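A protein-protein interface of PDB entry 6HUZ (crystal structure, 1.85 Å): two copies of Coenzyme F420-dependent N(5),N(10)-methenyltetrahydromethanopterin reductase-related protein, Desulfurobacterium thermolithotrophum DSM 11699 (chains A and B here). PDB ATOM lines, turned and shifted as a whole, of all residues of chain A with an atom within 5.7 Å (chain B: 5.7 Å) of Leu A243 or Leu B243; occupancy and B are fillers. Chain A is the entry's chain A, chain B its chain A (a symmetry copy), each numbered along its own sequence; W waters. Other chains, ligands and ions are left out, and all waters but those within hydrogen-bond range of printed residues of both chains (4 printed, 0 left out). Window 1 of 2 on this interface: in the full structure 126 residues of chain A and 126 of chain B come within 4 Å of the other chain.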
ATOM      1  N   THR A 209      -5.019  27.028  21.420  1.00  0.00           N
ATOM      2  CA  THR A 209      -3.862  26.461  22.103  1.00  0.00           C
ATOM      3  C   THR A 209      -4.306  25.368  23.072  1.00  0.00           C
ATOM      4  O   THR A 209      -3.634  24.329  23.218  1.00  0.00           O
ATOM      5  CB  THR A 209      -3.091  27.576  22.818  1.00  0.00           C
ATOM      6  OG1 THR A 209      -3.973  28.362  23.609  1.00  0.00           O
ATOM      7  CG2 THR A 209      -2.452  28.513  21.853  1.00  0.00           C
ATOM      8  N   THR A 210      -5.427  25.591  23.748  1.00  0.00           N
ATOM      9  CA  THR A 210      -5.931  24.614  24.725  1.00  0.00           C
ATOM     10  C   THR A 210      -6.211  23.259  24.030  1.00  0.00           C
ATOM     11  O   THR A 210      -5.697  22.218  24.436  1.00  0.00           O
ATOM     12  CB  THR A 210      -7.217  25.132  25.423  1.00  0.00           C
ATOM     13  OG1 THR A 210      -6.920  26.301  26.170  1.00  0.00           O
ATOM     14  CG2 THR A 210      -7.821  24.085  26.392  1.00  0.00           C
ATOM     15  N   ALA A 213      -2.911  21.577  22.312  1.00  0.00           N
ATOM     16  CA  ALA A 213      -2.056  20.988  23.359  1.00  0.00           C
ATOM     17  C   ALA A 213      -2.691  19.745  24.003  1.00  0.00           C
ATOM     18  O   ALA A 213      -2.020  18.739  24.276  1.00  0.00           O
ATOM     19  CB  ALA A 213      -1.766  22.045  24.420  1.00  0.00           C
ATOM     20  N   ALA A 217      -1.313  16.005  23.703  1.00  0.00           N
ATOM     21  CA  ALA A 217      -0.990  15.190  24.888  1.00  0.00           C
ATOM     22  C   ALA A 217      -1.632  13.828  24.759  1.00  0.00           C
ATOM     23  O   ALA A 217      -1.043  12.833  25.189  1.00  0.00           O
ATOM     24  CB  ALA A 217      -1.488  15.859  26.153  1.00  0.00           C
ATOM     25  N   GLN A 238       5.986  13.698  31.588  1.00  0.00           N
ATOM     26  CA  GLN A 238       6.419  14.343  30.335  1.00  0.00           C
ATOM     27  C   GLN A 238       5.389  15.369  29.841  1.00  0.00           C
ATOM     28  O   GLN A 238       5.784  16.465  29.463  1.00  0.00           O
ATOM     29  CB  GLN A 238       6.667  13.294  29.248  1.00  0.00           C
ATOM     30  CG  GLN A 238       7.934  12.472  29.499  1.00  0.00           C
ATOM     31  CD  GLN A 238       9.198  13.260  29.283  1.00  0.00           C
ATOM     32  OE1 GLN A 238       9.328  14.050  28.316  1.00  0.00           O
ATOM     33  NE2 GLN A 238      10.172  13.073  30.163  1.00  0.00           N
ATOM     34  N   ILE A 239       4.097  15.049  29.872  1.00  0.00           N
ATOM     35  CA  ILE A 239       3.046  16.017  29.437  1.00  0.00           C
ATOM     36  C   ILE A 239       3.080  17.244  30.361  1.00  0.00           C
ATOM     37  O   ILE A 239       3.161  18.358  29.881  1.00  0.00           O
ATOM     38  CB  ILE A 239       1.635  15.366  29.492  1.00  0.00           C
ATOM     39  CG1 ILE A 239       1.529  14.250  28.432  1.00  0.00           C
ATOM     40  CG2 ILE A 239       0.490  16.436  29.290  1.00  0.00           C
ATOM     41  CD1 ILE A 239       0.453  13.292  28.710  1.00  0.00           C
ATOM     42  N   ALA A 240       3.016  17.024  31.676  1.00  0.00           N
ATOM     43  CA  ALA A 240       3.019  18.122  32.641  1.00  0.00           C
ATOM     44  C   ALA A 240       4.225  19.007  32.482  1.00  0.00           C
ATOM     45  O   ALA A 240       4.091  20.223  32.456  1.00  0.00           O
ATOM     46  CB  ALA A 240       2.953  17.574  34.071  1.00  0.00           C
ATOM     47  N   GLN A 241       5.418  18.406  32.373  1.00  0.00           N
ATOM     48  CA  GLN A 241       6.629  19.171  32.250  1.00  0.00           C
ATOM     49  C   GLN A 241       6.657  19.986  30.995  1.00  0.00           C
ATOM     50  O   GLN A 241       7.067  21.120  31.080  1.00  0.00           O
ATOM     51  CB  GLN A 241       7.886  18.262  32.257  1.00  0.00           C
ATOM     52  CG  GLN A 241       9.187  19.081  32.265  1.00  0.00           C
ATOM     53  CD  GLN A 241      10.460  18.250  32.206  1.00  0.00           C
ATOM     54  OE1 GLN A 241      11.347  18.371  33.044  1.00  0.00           O
ATOM     55  NE2 GLN A 241      10.610  17.407  31.206  1.00  0.00           N
ATOM     56  N   SER A 242       6.351  19.388  29.824  1.00  0.00           N
ATOM     57  CA  SER A 242       6.425  20.109  28.564  1.00  0.00           C
ATOM     58  C   SER A 242       5.581  21.359  28.629  1.00  0.00           C
ATOM     59  O   SER A 242       6.055  22.444  28.292  1.00  0.00           O
ATOM     60  CB  SER A 242       5.913  19.246  27.387  1.00  0.00           C
ATOM     61  OG  SER A 242       6.779  18.169  27.055  1.00  0.00           O
ATOM     62  N   LEU A 243       4.318  21.201  29.040  1.00  0.00           N
ATOM     63  CA  LEU A 243       3.389  22.322  29.067  1.00  0.00           C
ATOM     64  C   LEU A 243       3.720  23.364  30.122  1.00  0.00           C
ATOM     65  O   LEU A 243       3.579  24.550  29.825  1.00  0.00           O
ATOM     66  CB  LEU A 243       1.947  21.819  29.167  1.00  0.00           C
ATOM     67  CG  LEU A 243       1.567  20.795  28.074  1.00  0.00           C
ATOM     68  CD1 LEU A 243       0.132  20.350  28.223  1.00  0.00           C
ATOM     69  CD2 LEU A 243       1.892  21.311  26.645  1.00  0.00           C
ATOM     70  N   GLN A 244       4.187  22.953  31.313  1.00  0.00           N
ATOM     71  CA  GLN A 244       4.582  23.908  32.364  1.00  0.00           C
ATOM     72  C   GLN A 244       5.754  24.734  31.817  1.00  0.00           C
ATOM     73  O   GLN A 244       5.783  25.939  31.981  1.00  0.00           O
ATOM     74  CB  GLN A 244       5.065  23.158  33.612  1.00  0.00           C
ATOM     75  CG  GLN A 244       5.424  24.021  34.818  1.00  0.00           C
ATOM     76  CD  GLN A 244       4.298  24.918  35.269  1.00  0.00           C
ATOM     77  OE1 GLN A 244       3.405  24.518  36.030  1.00  0.00           O
ATOM     78  NE2 GLN A 244       4.313  26.151  34.810  1.00  0.00           N
ATOM     79  N   VAL A 245       6.741  24.072  31.184  1.00  0.00           N
ATOM     80  CA  VAL A 245       7.901  24.783  30.646  1.00  0.00           C
ATOM     81  C   VAL A 245       7.506  25.837  29.606  1.00  0.00           C
ATOM     82  O   VAL A 245       7.969  26.980  29.688  1.00  0.00           O
ATOM     83  CB  VAL A 245       8.956  23.796  30.103  1.00  0.00           C
ATOM     84  CG1 VAL A 245       9.976  24.495  29.211  1.00  0.00           C
ATOM     85  CG2 VAL A 245       9.651  23.087  31.258  1.00  0.00           C
ATOM     86  N   ILE A 246       6.684  25.462  28.623  1.00  0.00           N
ATOM     87  CA  ILE A 246       6.273  26.423  27.598  1.00  0.00           C
ATOM     88  C   ILE A 246       5.529  27.560  28.263  1.00  0.00           C
ATOM     89  O   ILE A 246       5.836  28.697  27.990  1.00  0.00           O
ATOM     90  CB  ILE A 246       5.397  25.790  26.478  1.00  0.00           C
ATOM     91  CG1 ILE A 246       6.257  24.763  25.660  1.00  0.00           C
ATOM     92  CG2 ILE A 246       4.826  26.902  25.550  1.00  0.00           C
ATOM     93  CD1 ILE A 246       5.396  23.863  24.791  1.00  0.00           C
ATOM     94  N   SER A 247       4.559  27.260  29.125  1.00  0.00           N
ATOM     95  CA  SER A 247       3.771  28.307  29.820  1.00  0.00           C
ATOM     96  C   SER A 247       4.708  29.274  30.605  1.00  0.00           C
ATOM     97  O   SER A 247       4.552  30.491  30.513  1.00  0.00           O
ATOM     98  CB  SER A 247       2.798  27.657  30.815  1.00  0.00           C
ATOM     99  OG  SER A 247       1.950  28.672  31.330  1.00  0.00           O
ATOM    100  N   SER A 248       5.679  28.720  31.380  1.00  0.00           N
ATOM    101  CA  SER A 248       6.607  29.533  32.180  1.00  0.00           C
ATOM    102  C   SER A 248       7.439  30.468  31.296  1.00  0.00           C
ATOM    103  O   SER A 248       7.674  31.633  31.650  1.00  0.00           O
ATOM    104  CB  SER A 248       7.579  28.640  32.979  1.00  0.00           C
ATOM    105  OG  SER A 248       6.829  27.856  33.906  1.00  0.00           O
ATOM    106  N   THR B 209       4.626  16.371  22.822  1.00  0.00           N
ATOM    107  CA  THR B 209       3.752  17.364  23.435  1.00  0.00           C
ATOM    108  C   THR B 209       4.389  18.749  23.353  1.00  0.00           C
ATOM    109  O   THR B 209       3.698  19.760  23.122  1.00  0.00           O
ATOM    110  CB  THR B 209       3.452  16.961  24.883  1.00  0.00           C
ATOM    111  OG1 THR B 209       4.658  16.663  25.575  1.00  0.00           O
ATOM    112  CG2 THR B 209       2.618  15.729  24.952  1.00  0.00           C
ATOM    113  N   THR B 210       5.701  18.813  23.550  1.00  0.00           N
ATOM    114  CA  THR B 210       6.411  20.101  23.518  1.00  0.00           C
ATOM    115  C   THR B 210       6.237  20.772  22.133  1.00  0.00           C
ATOM    116  O   THR B 210       5.789  21.913  22.031  1.00  0.00           O
ATOM    117  CB  THR B 210       7.918  19.918  23.837  1.00  0.00           C
ATOM    118  OG1 THR B 210       8.073  19.429  25.160  1.00  0.00           O
ATOM    119  CG2 THR B 210       8.709  21.246  23.720  1.00  0.00           C
ATOM    120  N   ALA B 213       2.351  21.571  21.166  1.00  0.00           N
ATOM    121  CA  ALA B 213       1.889  22.752  21.918  1.00  0.00           C
ATOM    122  C   ALA B 213       2.560  24.049  21.442  1.00  0.00           C
ATOM    123  O   ALA B 213       1.923  25.106  21.321  1.00  0.00           O
ATOM    124  CB  ALA B 213       2.154  22.532  23.404  1.00  0.00           C
ATOM    125  N   ALA B 217       0.718  27.089  19.614  1.00  0.00           N
ATOM    126  CA  ALA B 217       0.768  28.467  20.137  1.00  0.00           C
ATOM    127  C   ALA B 217       1.139  29.420  19.025  1.00  0.00           C
ATOM    128  O   ALA B 217       0.637  30.547  18.995  1.00  0.00           O
ATOM    129  CB  ALA B 217       1.786  28.581  21.254  1.00  0.00           C
ATOM    130  N   GLN B 238      -3.290  34.359  26.814  1.00  0.00           N
ATOM    131  CA  GLN B 238      -4.080  33.175  26.430  1.00  0.00           C
ATOM    132  C   GLN B 238      -3.194  31.932  26.265  1.00  0.00           C
ATOM    133  O   GLN B 238      -3.564  30.876  26.761  1.00  0.00           O
ATOM    134  CB  GLN B 238      -4.849  33.440  25.132  1.00  0.00           C
ATOM    135  CG  GLN B 238      -6.019  34.409  25.326  1.00  0.00           C
ATOM    136  CD  GLN B 238      -7.162  33.802  26.094  1.00  0.00           C
ATOM    137  OE1 GLN B 238      -7.548  32.625  25.887  1.00  0.00           O
ATOM    138  NE2 GLN B 238      -7.746  34.576  26.998  1.00  0.00           N
ATOM    139  N   ILE B 239      -2.037  32.049  25.617  1.00  0.00           N
ATOM    140  CA  ILE B 239      -1.116  30.885  25.453  1.00  0.00           C
ATOM    141  C   ILE B 239      -0.646  30.418  26.840  1.00  0.00           C
ATOM    142  O   ILE B 239      -0.763  29.249  27.154  1.00  0.00           O
ATOM    143  CB  ILE B 239       0.118  31.270  24.591  1.00  0.00           C
ATOM    144  CG1 ILE B 239      -0.323  31.561  23.141  1.00  0.00           C
ATOM    145  CG2 ILE B 239       1.226  30.144  24.620  1.00  0.00           C
ATOM    146  CD1 ILE B 239       0.650  32.363  22.393  1.00  0.00           C
ATOM    147  N   ALA B 240      -0.119  31.337  27.651  1.00  0.00           N
ATOM    148  CA  ALA B 240       0.380  30.995  28.981  1.00  0.00           C
ATOM    149  C   ALA B 240      -0.678  30.335  29.825  1.00  0.00           C
ATOM    150  O   ALA B 240      -0.413  29.315  30.448  1.00  0.00           O
ATOM    151  CB  ALA B 240       0.912  32.246  29.690  1.00  0.00           C
ATOM    152  N   GLN B 241      -1.887  30.909  29.854  1.00  0.00           N
ATOM    153  CA  GLN B 241      -2.951  30.367  30.656  1.00  0.00           C
ATOM    154  C   GLN B 241      -3.349  28.995  30.214  1.00  0.00           C
ATOM    155  O   GLN B 241      -3.552  28.173  31.076  1.00  0.00           O
ATOM    156  CB  GLN B 241      -4.215  31.267  30.619  1.00  0.00           C
ATOM    157  CG  GLN B 241      -5.303  30.767  31.582  1.00  0.00           C
ATOM    158  CD  GLN B 241      -6.597  31.568  31.546  1.00  0.00           C
ATOM    159  OE1 GLN B 241      -7.079  32.056  32.561  1.00  0.00           O
ATOM    160  NE2 GLN B 241      -7.217  31.701  30.392  1.00  0.00           N
ATOM    161  N   SER B 242      -3.585  28.776  28.903  1.00  0.00           N
ATOM    162  CA  SER B 242      -4.038  27.482  28.421  1.00  0.00           C
ATOM    163  C   SER B 242      -3.084  26.399  28.861  1.00  0.00           C
ATOM    164  O   SER B 242      -3.512  25.384  29.412  1.00  0.00           O
ATOM    165  CB  SER B 242      -4.120  27.450  26.877  1.00  0.00           C
ATOM    166  OG  SER B 242      -5.173  28.244  26.348  1.00  0.00           O
ATOM    167  N   LEU B 243      -1.790  26.604  28.595  1.00  0.00           N
ATOM    168  CA  LEU B 243      -0.788  25.592  28.902  1.00  0.00           C
ATOM    169  C   LEU B 243      -0.564  25.387  30.391  1.00  0.00           C
ATOM    170  O   LEU B 243      -0.399  24.237  30.796  1.00  0.00           O
ATOM    171  CB  LEU B 243       0.511  25.880  28.145  1.00  0.00           C
ATOM    172  CG  LEU B 243       0.320  26.042  26.620  1.00  0.00           C
ATOM    173  CD1 LEU B 243       1.637  26.310  25.934  1.00  0.00           C
ATOM    174  CD2 LEU B 243      -0.454  24.849  25.992  1.00  0.00           C
ATOM    175  N   GLN B 244      -0.594  26.458  31.204  1.00  0.00           N
ATOM    176  CA  GLN B 244      -0.441  26.329  32.663  1.00  0.00           C
ATOM    177  C   GLN B 244      -1.620  25.491  33.176  1.00  0.00           C
ATOM    178  O   GLN B 244      -1.435  24.609  33.993  1.00  0.00           O
ATOM    179  CB  GLN B 244      -0.506  27.709  33.330  1.00  0.00           C
ATOM    180  CG  GLN B 244      -0.274  27.738  34.837  1.00  0.00           C
ATOM    181  CD  GLN B 244       1.042  27.126  35.253  1.00  0.00           C
ATOM    182  OE1 GLN B 244       2.099  27.773  35.244  1.00  0.00           O
ATOM    183  NE2 GLN B 244       1.008  25.865  35.625  1.00  0.00           N
ATOM    184  N   VAL B 245      -2.848  25.791  32.710  1.00  0.00           N
ATOM    185  CA  VAL B 245      -4.026  25.052  33.160  1.00  0.00           C
ATOM    186  C   VAL B 245      -3.926  23.554  32.851  1.00  0.00           C
ATOM    187  O   VAL B 245      -4.177  22.729  33.737  1.00  0.00           O
ATOM    188  CB  VAL B 245      -5.322  25.676  32.600  1.00  0.00           C
ATOM    189  CG1 VAL B 245      -6.508  24.727  32.731  1.00  0.00           C
ATOM    190  CG2 VAL B 245      -5.612  26.996  33.302  1.00  0.00           C
ATOM    191  N   ILE B 246      -3.589  23.198  31.609  1.00  0.00           N
ATOM    192  CA  ILE B 246      -3.480  21.782  31.252  1.00  0.00           C
ATOM    193  C   ILE B 246      -2.405  21.144  32.105  1.00  0.00           C
ATOM    194  O   ILE B 246      -2.648  20.102  32.669  1.00  0.00           O
ATOM    195  CB  ILE B 246      -3.177  21.550  29.744  1.00  0.00           C
ATOM    196  CG1 ILE B 246      -4.402  22.026  28.886  1.00  0.00           C
ATOM    197  CG2 ILE B 246      -2.865  20.047  29.483  1.00  0.00           C
ATOM    198  CD1 ILE B 246      -4.052  22.155  27.414  1.00  0.00           C
ATOM    199  N   SER B 247      -1.226  21.758  32.197  1.00  0.00           N
ATOM    200  CA  SER B 247      -0.111  21.205  33.004  1.00  0.00           C
ATOM    201  C   SER B 247      -0.554  20.982  34.481  1.00  0.00           C
ATOM    202  O   SER B 247      -0.294  19.921  35.048  1.00  0.00           O
ATOM    203  CB  SER B 247       1.077  22.179  32.993  1.00  0.00           C
ATOM    204  OG  SER B 247       2.176  21.541  33.627  1.00  0.00           O
ATOM    205  N   SER B 248      -1.221  21.994  35.098  1.00  0.00           N
ATOM    206  CA  SER B 248      -1.670  21.904  36.495  1.00  0.00           C
ATOM    207  C   SER B 248      -2.651  20.744  36.696  1.00  0.00           C
ATOM    208  O   SER B 248      -2.589  20.028  37.707  1.00  0.00           O
ATOM    209  CB  SER B 248      -2.371  23.205  36.938  1.00  0.00           C
ATOM    210  OG  SER B 248      -1.431  24.277  36.886  1.00  0.00           O
HETATM  211  O   HOH W   1      -1.034  24.352  21.382  1.00  0.00           O
HETATM  212  O   HOH W   2       0.622  19.019  22.776  1.00  0.00           O
HETATM  213  O   HOH W   3       2.772  30.397  33.550  1.00  0.00           O
HETATM  214  O   HOH W   4       2.473  21.506  36.540  1.00  0.00           O
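Among the printed residues, pairs that only touch across the chains: Leu A243 with Ile B246 (3.3 Å), Ile A246 with Leu B243 (3.3 Å), Ile A246 with Thr B210 (3.4 Å), Thr A210 with Ile B246 (3.4 Å), Ala A213 with Leu B243 (3.5 Å), Leu A243 with Ala B213 (3.5 Å), Ala A217 with Thr B209 (3.6 Å), Thr A209 with Ala B217 (3.6 Å), Leu A243 with Leu B243 (3.7 Å), Ala A213 with Ile B246 (3.8 Å), Ile A246 with Ala B213 (3.8 Å), Thr A209 with Ile B239 (3.9 Å), Ile A239 with Thr B209 (3.9 Å), Ser A247 with Leu B243 (3.9 Å) and Leu A243 with Ser B247 (3.9 Å).
Thr A209 touches Ser B242, and with the chains exchanged Ser A242 touches Thr B209. Ala A213 touches Ile B246, and with the chains exchanged Ile A246 touches Ala B213. Ala A240 touches Ser B247, and with the chains exchanged Ser A247 touches Ala B240. Leu A243 touches its own counterpart, Leu B243.
Of the 15 printed residues of chain B, 11 touch a printed residue of chain A. Of the 15 printed residues of chain A, 11 touch a printed residue of chain B. Along chain A the printed residues that touch a printed residue of chain B span positions 209 to 247.
The backbone carbonyl oxygen of Gln A238 sits at hydrogen-bond distance from the side-chain hydroxyl of Ser A242, at 3.1 Å. The backbone carbonyl oxygen (O) of Gln A244 sits at hydrogen-bond distance from the side-chain hydroxyl (OG) of Ser A248 (2.9 Å). The side-chain hydroxyl of Ser B242 lies within hydrogen-bond range of the backbone carbonyl oxygen of Gln B238 (3.1 Å). The backbone carbonyl oxygen (O) of Gln B244 sits at hydrogen-bond distance from the side-chain hydroxyl (OG) of Ser B248 (2.9 Å).
OG1 of Thr A209 lies within hydrogen-bond range of OG of Ser B242, at 3.0 Å. OG1 of Thr A210 is in hydrogen-bond range of OG of Ser B242 (2.6 Å). OG of Ser B247 is in hydrogen-bond range of O of Ala A240. The side-chain hydroxyl (OG) of Ser A242 sits at hydrogen-bond distance from the side-chain hydroxyl (OG1) of Thr B209, at 3.0 Å. OG of Ser A242 lies within hydrogen-bond range of OG1 of Thr B210 (2.6 Å). The side-chain amide oxygen (OE1) of Gln A244 is in hydrogen-bond range of the side-chain amide nitrogen (NE2) of Gln B244. OG of Ser B247 sits close to N of Gln A244 (3.4 Å). The side-chain hydroxyl of Ser A247 lies within hydrogen-bond range of the backbone carbonyl oxygen of Ala B240 (2.6 Å). N of Gln B244 lies close to OG of Ser A247 (3.4 Å).
Water W3 bridges OG of Ser A247 and OE1 of Gln B244. Water W4 lies within hydrogen-bond range of the side-chain hydroxyl (OG) of Ser B247 (2.9 Å) and the side-chain amide oxygen (OE1) of Gln A244 (3.2 Å). Water W1 lies within hydrogen-bond range of O of Ala B213 (3.1 Å), O of Thr A209 (3.2 Å) and N of Ala A213 (3.5 Å). Water W2 lies within hydrogen-bond range of the backbone carbonyl oxygen (O) of Ala A213 (3.1 Å), the backbone carbonyl oxygen (O) of Thr B209 (3.2 Å) and the backbone NH (N) of Ala B213 (3.5 Å).
Printed residues of chain B within 4 Å of Leu A243: Ala B213 (3.5 Å), Leu B243 (3.7 Å), Ile B246 (3.3 Å) and Ser B247 (3.9 Å). Of the printed residues of chain A, Leu B243 touches Ala A213, Leu A243, Ile A246 and Ser A247. Of the printed residues of chain A, Ser B247 touches Ala A240 (2.6 Å), Leu A243 (3.9 Å) and Gln A244 (3.3 Å). Printed residues of chain B within 4 Å of Thr A210: Ser B242 (2.6 Å) and Ile B246 (3.4 Å). Gln B241 touches none of the printed residues of chain A. Gln B238 touches none of the printed residues of chain A. The nearest residue of chain B that does not touch Leu A243 is Thr B209 (4.3 Å).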
